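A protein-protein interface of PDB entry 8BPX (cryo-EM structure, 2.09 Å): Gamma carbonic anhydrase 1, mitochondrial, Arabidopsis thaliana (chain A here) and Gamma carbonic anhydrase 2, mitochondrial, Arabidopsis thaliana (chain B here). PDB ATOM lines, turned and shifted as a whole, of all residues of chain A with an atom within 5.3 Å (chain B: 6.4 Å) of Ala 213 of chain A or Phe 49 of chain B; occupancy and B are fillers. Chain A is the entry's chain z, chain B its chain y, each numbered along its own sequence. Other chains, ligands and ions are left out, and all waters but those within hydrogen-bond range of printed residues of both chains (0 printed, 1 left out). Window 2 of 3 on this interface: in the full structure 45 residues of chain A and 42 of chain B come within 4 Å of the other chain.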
ATOM      1  N   ASN A 209     -31.462  10.176 -28.811  1.00  0.00           N
ATOM      2  CA  ASN A 209     -30.055  10.258 -28.336  1.00  0.00           C
ATOM      3  C   ASN A 209     -29.947  11.149 -27.093  1.00  0.00           C
ATOM      4  O   ASN A 209     -29.239  10.752 -26.161  1.00  0.00           O
ATOM      5  CB  ASN A 209     -29.076  10.797 -29.384  1.00  0.00           C
ATOM      6  CG  ASN A 209     -29.138   9.993 -30.658  1.00  0.00           C
ATOM      7  OD1 ASN A 209     -29.560   8.845 -30.638  1.00  0.00           O
ATOM      8  ND2 ASN A 209     -28.818  10.626 -31.768  1.00  0.00           N
ATOM      9  N   LEU A 210     -30.595  12.293 -27.130  1.00  0.00           N
ATOM     10  CA  LEU A 210     -30.636  13.200 -25.957  1.00  0.00           C
ATOM     11  C   LEU A 210     -31.288  12.441 -24.786  1.00  0.00           C
ATOM     12  O   LEU A 210     -30.721  12.507 -23.732  1.00  0.00           O
ATOM     13  CB  LEU A 210     -31.376  14.474 -26.379  1.00  0.00           C
ATOM     14  CG  LEU A 210     -31.347  15.683 -25.448  1.00  0.00           C
ATOM     15  CD1 LEU A 210     -29.921  16.123 -25.155  1.00  0.00           C
ATOM     16  CD2 LEU A 210     -32.126  16.824 -26.086  1.00  0.00           C
ATOM     17  N   ALA A 211     -32.417  11.757 -25.018  1.00  0.00           N
ATOM     18  CA  ALA A 211     -33.066  10.889 -23.993  1.00  0.00           C
ATOM     19  C   ALA A 211     -31.992   9.986 -23.378  1.00  0.00           C
ATOM     20  O   ALA A 211     -31.835  10.096 -22.196  1.00  0.00           O
ATOM     21  CB  ALA A 211     -34.286  10.133 -24.493  1.00  0.00           C
ATOM     22  N   GLN A 212     -31.250   9.238 -24.220  1.00  0.00           N
ATOM     23  CA  GLN A 212     -30.190   8.358 -23.718  1.00  0.00           C
ATOM     24  C   GLN A 212     -29.263   9.094 -22.756  1.00  0.00           C
ATOM     25  O   GLN A 212     -28.955   8.597 -21.660  1.00  0.00           O
ATOM     26  CB  GLN A 212     -29.390   7.776 -24.884  1.00  0.00           C
ATOM     27  CG  GLN A 212     -29.816   6.397 -25.327  1.00  0.00           C
ATOM     28  CD  GLN A 212     -31.303   6.177 -25.227  1.00  0.00           C
ATOM     29  OE1 GLN A 212     -32.060   6.543 -26.123  1.00  0.00           O
ATOM     30  NE2 GLN A 212     -31.732   5.552 -24.139  1.00  0.00           N
ATOM     31  N   ALA A 213     -28.810  10.284 -23.154  1.00  0.00           N
ATOM     32  CA  ALA A 213     -27.895  11.035 -22.296  1.00  0.00           C
ATOM     33  C   ALA A 213     -28.543  11.381 -20.956  1.00  0.00           C
ATOM     34  O   ALA A 213     -27.923  11.223 -19.894  1.00  0.00           O
ATOM     35  CB  ALA A 213     -27.419  12.302 -23.005  1.00  0.00           C
ATOM     36  N   HIS A 214     -29.799  11.832 -20.982  1.00  0.00           N
ATOM     37  CA  HIS A 214     -30.460  12.217 -19.737  1.00  0.00           C
ATOM     38  C   HIS A 214     -30.784  11.010 -18.864  1.00  0.00           C
ATOM     39  O   HIS A 214     -30.758  11.116 -17.634  1.00  0.00           O
ATOM     40  CB  HIS A 214     -31.726  13.017 -20.032  1.00  0.00           C
ATOM     41  CG  HIS A 214     -31.466  14.458 -20.341  1.00  0.00           C
ATOM     42  ND1 HIS A 214     -31.766  15.474 -19.460  1.00  0.00           N
ATOM     43  CD2 HIS A 214     -30.927  15.052 -21.432  1.00  0.00           C
ATOM     44  CE1 HIS A 214     -31.424  16.633 -19.996  1.00  0.00           C
ATOM     45  NE2 HIS A 214     -30.913  16.403 -21.192  1.00  0.00           N
ATOM     46  N   ALA A 215     -31.106   9.866 -19.472  1.00  0.00           N
ATOM     47  CA  ALA A 215     -31.346   8.656 -18.695  1.00  0.00           C
ATOM     48  C   ALA A 215     -30.079   8.207 -17.988  1.00  0.00           C
ATOM     49  O   ALA A 215     -30.124   7.788 -16.826  1.00  0.00           O
ATOM     50  CB  ALA A 215     -31.884   7.543 -19.594  1.00  0.00           C
ATOM     51  N   ALA A 216     -28.936   8.290 -18.674  1.00  0.00           N
ATOM     52  CA  ALA A 216     -27.675   7.975 -18.011  1.00  0.00           C
ATOM     53  C   ALA A 216     -27.382   8.962 -16.884  1.00  0.00           C
ATOM     54  O   ALA A 216     -26.913   8.567 -15.810  1.00  0.00           O
ATOM     55  CB  ALA A 216     -26.535   7.954 -19.028  1.00  0.00           C
ATOM     56  N   GLU A 217     -27.652  10.251 -17.109  1.00  0.00           N
ATOM     57  CA  GLU A 217     -27.444  11.246 -16.059  1.00  0.00           C
ATOM     58  C   GLU A 217     -28.283  10.931 -14.822  1.00  0.00           C
ATOM     59  O   GLU A 217     -27.769  10.904 -13.699  1.00  0.00           O
ATOM     60  CB  GLU A 217     -27.784  12.643 -16.584  1.00  0.00           C
ATOM     61  CG  GLU A 217     -26.618  13.428 -17.187  1.00  0.00           C
ATOM     62  CD  GLU A 217     -25.382  13.469 -16.309  1.00  0.00           C
ATOM     63  OE1 GLU A 217     -25.511  13.449 -15.068  1.00  0.00           O
ATOM     64  OE2 GLU A 217     -24.268  13.536 -16.866  1.00  0.00           O
ATOM     65  N   ASN A 218     -29.579  10.683 -15.015  1.00  0.00           N
ATOM     66  CA  ASN A 218     -30.476  10.467 -13.884  1.00  0.00           C
ATOM     67  C   ASN A 218     -30.192   9.147 -13.179  1.00  0.00           C
ATOM     68  O   ASN A 218     -30.412   9.036 -11.970  1.00  0.00           O
ATOM     69  CB  ASN A 218     -31.933  10.516 -14.349  1.00  0.00           C
ATOM     70  CG  ASN A 218     -32.461  11.936 -14.480  1.00  0.00           C
ATOM     71  OD1 ASN A 218     -32.787  12.582 -13.487  1.00  0.00           O
ATOM     72  ND2 ASN A 218     -32.552  12.421 -15.711  1.00  0.00           N
ATOM     73  N   ASN B  47     -26.169  17.977 -13.754  1.00  0.00           N
ATOM     74  CA  ASN B  47     -25.242  18.098 -14.866  1.00  0.00           C
ATOM     75  C   ASN B  47     -25.754  17.315 -16.065  1.00  0.00           C
ATOM     76  O   ASN B  47     -26.515  16.354 -15.926  1.00  0.00           O
ATOM     77  CB  ASN B  47     -23.859  17.569 -14.487  1.00  0.00           C
ATOM     78  CG  ASN B  47     -23.333  18.176 -13.216  1.00  0.00           C
ATOM     79  OD1 ASN B  47     -22.757  19.257 -13.224  1.00  0.00           O
ATOM     80  ND2 ASN B  47     -23.527  17.478 -12.106  1.00  0.00           N
ATOM     81  N   VAL B  48     -25.334  17.742 -17.250  1.00  0.00           N
ATOM     82  CA  VAL B  48     -25.466  16.932 -18.456  1.00  0.00           C
ATOM     83  C   VAL B  48     -24.401  17.399 -19.437  1.00  0.00           C
ATOM     84  O   VAL B  48     -24.125  18.597 -19.542  1.00  0.00           O
ATOM     85  CB  VAL B  48     -26.890  17.009 -19.057  1.00  0.00           C
ATOM     86  CG1 VAL B  48     -27.259  18.436 -19.416  1.00  0.00           C
ATOM     87  CG2 VAL B  48     -27.021  16.079 -20.256  1.00  0.00           C
ATOM     88  N   PHE B  49     -23.784  16.444 -20.132  1.00  0.00           N
ATOM     89  CA  PHE B  49     -22.706  16.730 -21.082  1.00  0.00           C
ATOM     90  C   PHE B  49     -21.579  17.515 -20.418  1.00  0.00           C
ATOM     91  O   PHE B  49     -20.960  18.390 -21.026  1.00  0.00           O
ATOM     92  CB  PHE B  49     -23.233  17.478 -22.307  1.00  0.00           C
ATOM     93  CG  PHE B  49     -24.296  16.741 -23.056  1.00  0.00           C
ATOM     94  CD1 PHE B  49     -24.098  15.430 -23.454  1.00  0.00           C
ATOM     95  CD2 PHE B  49     -25.489  17.362 -23.376  1.00  0.00           C
ATOM     96  CE1 PHE B  49     -25.073  14.748 -24.150  1.00  0.00           C
ATOM     97  CE2 PHE B  49     -26.467  16.689 -24.073  1.00  0.00           C
ATOM     98  CZ  PHE B  49     -26.260  15.376 -24.459  1.00  0.00           C
ATOM     99  N   ASP B  50     -21.310  17.192 -19.151  1.00  0.00           N
ATOM    100  CA  ASP B  50     -20.281  17.869 -18.359  1.00  0.00           C
ATOM    101  C   ASP B  50     -20.501  19.379 -18.315  1.00  0.00           C
ATOM    102  O   ASP B  50     -19.557  20.166 -18.396  1.00  0.00           O
ATOM    103  CB  ASP B  50     -18.875  17.540 -18.870  1.00  0.00           C
ATOM    104  CG  ASP B  50     -18.463  16.113 -18.574  1.00  0.00           C
ATOM    105  OD1 ASP B  50     -19.122  15.459 -17.738  1.00  0.00           O
ATOM    106  OD2 ASP B  50     -17.476  15.641 -19.178  1.00  0.00           O
ATOM    107  N   LYS B  51     -21.760  19.791 -18.199  1.00  0.00           N
ATOM    108  CA  LYS B  51     -22.116  21.185 -17.978  1.00  0.00           C
ATOM    109  C   LYS B  51     -22.850  21.294 -16.650  1.00  0.00           C
ATOM    110  O   LYS B  51     -23.845  20.599 -16.429  1.00  0.00           O
ATOM    111  CB  LYS B  51     -22.984  21.732 -19.116  1.00  0.00           C
ATOM    112  CG  LYS B  51     -22.281  21.811 -20.456  1.00  0.00           C
ATOM    113  CD  LYS B  51     -21.378  23.033 -20.533  1.00  0.00           C
ATOM    114  CE  LYS B  51     -20.365  22.905 -21.659  1.00  0.00           C
ATOM    115  NZ  LYS B  51     -20.447  24.042 -22.615  1.00  0.00           N
ATOM    116  N   GLY B  87     -30.855  23.447 -20.057  1.00  0.00           N
ATOM    117  CA  GLY B  87     -29.739  23.915 -20.858  1.00  0.00           C
ATOM    118  C   GLY B  87     -28.829  22.789 -21.304  1.00  0.00           C
ATOM    119  O   GLY B  87     -27.656  22.760 -20.925  1.00  0.00           O
ATOM    120  N   ASP B  88     -29.344  21.855 -22.103  1.00  0.00           N
ATOM    121  CA  ASP B  88     -28.570  20.665 -22.444  1.00  0.00           C
ATOM    122  C   ASP B  88     -27.841  20.768 -23.779  1.00  0.00           C
ATOM    123  O   ASP B  88     -26.679  20.370 -23.864  1.00  0.00           O
ATOM    124  CB  ASP B  88     -29.463  19.416 -22.443  1.00  0.00           C
ATOM    125  CG  ASP B  88     -30.770  19.616 -23.181  1.00  0.00           C
ATOM    126  OD1 ASP B  88     -30.931  20.637 -23.879  1.00  0.00           O
ATOM    127  OD2 ASP B  88     -31.642  18.735 -23.062  1.00  0.00           O
ATOM    128  N   VAL B  89     -28.431  21.293 -24.843  1.00  0.00           N
ATOM    129  CA  VAL B  89     -27.759  21.389 -26.189  1.00  0.00           C
ATOM    130  C   VAL B  89     -27.195  22.810 -26.413  1.00  0.00           C
ATOM    131  O   VAL B  89     -26.422  22.977 -27.298  1.00  0.00           O
ATOM    132  CB  VAL B  89     -28.686  20.926 -27.333  1.00  0.00           C
ATOM    133  CG1 VAL B  89     -29.173  19.508 -27.063  1.00  0.00           C
ATOM    134  CG2 VAL B  89     -29.885  21.847 -27.501  1.00  0.00           C
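The side-chain amide nitrogen (ND2) of Asn 218 of chain A is in hydrogen-bond range of the backbone carbonyl oxygen (O) of His 214 of chain A (2.9 Å).
Leu 210 of chain A touches Phe 49 of chain B (CD1 to CE2, 3.7 Å).
Asp 88 of chain B touches Leu 210 of chain A (OD2 to CD2, 3.6 Å).
CD1 of Leu 210 of chain A touches CG1 of Val 89 of chain B (3.96 Å).
CB of Ala 213 of chain A touches CE1 of Phe 49 of chain B, 3.6 Å away.
Glu 217 of chain A touches Val 48 of chain B.
Of the printed residues of chain B, Ala 213 of chain A touches Phe 49.
Of chain A, only Leu 210 and Ala 213 come within 4 Å of Phe 49 of chain B.
Printed residues of chain B within 4 Å of His 214 of chain A: Asp 88.
Of the printed residues of chain A, Asp 88 of chain B touches Leu 210 (3.6 Å) and His 214 (3.1 Å).
Of the printed residues of chain B, Leu 210 of chain A touches Phe 49 (3.7 Å), Asp 88 (3.6 Å) and Val 89 (3.96 Å).
The nearest residue of chain B that does not touch Ala 213 of chain A is Val 48 of chain B (4.7 Å).
A ring nitrogen (NE2) of His 214 of chain A sits at hydrogen-bond distance from the side-chain carboxylate of Asp 88 of chain B.
O of Asn 47 of chain B lies close to OE1 of Glu 217 of chain A.
Among the printed residues, 7 pairs touch across the chains.
Among the printed residues, no Asp or Glu carboxylate lies within 4 Å of a Lys or Arg side-chain nitrogen of the other chain.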
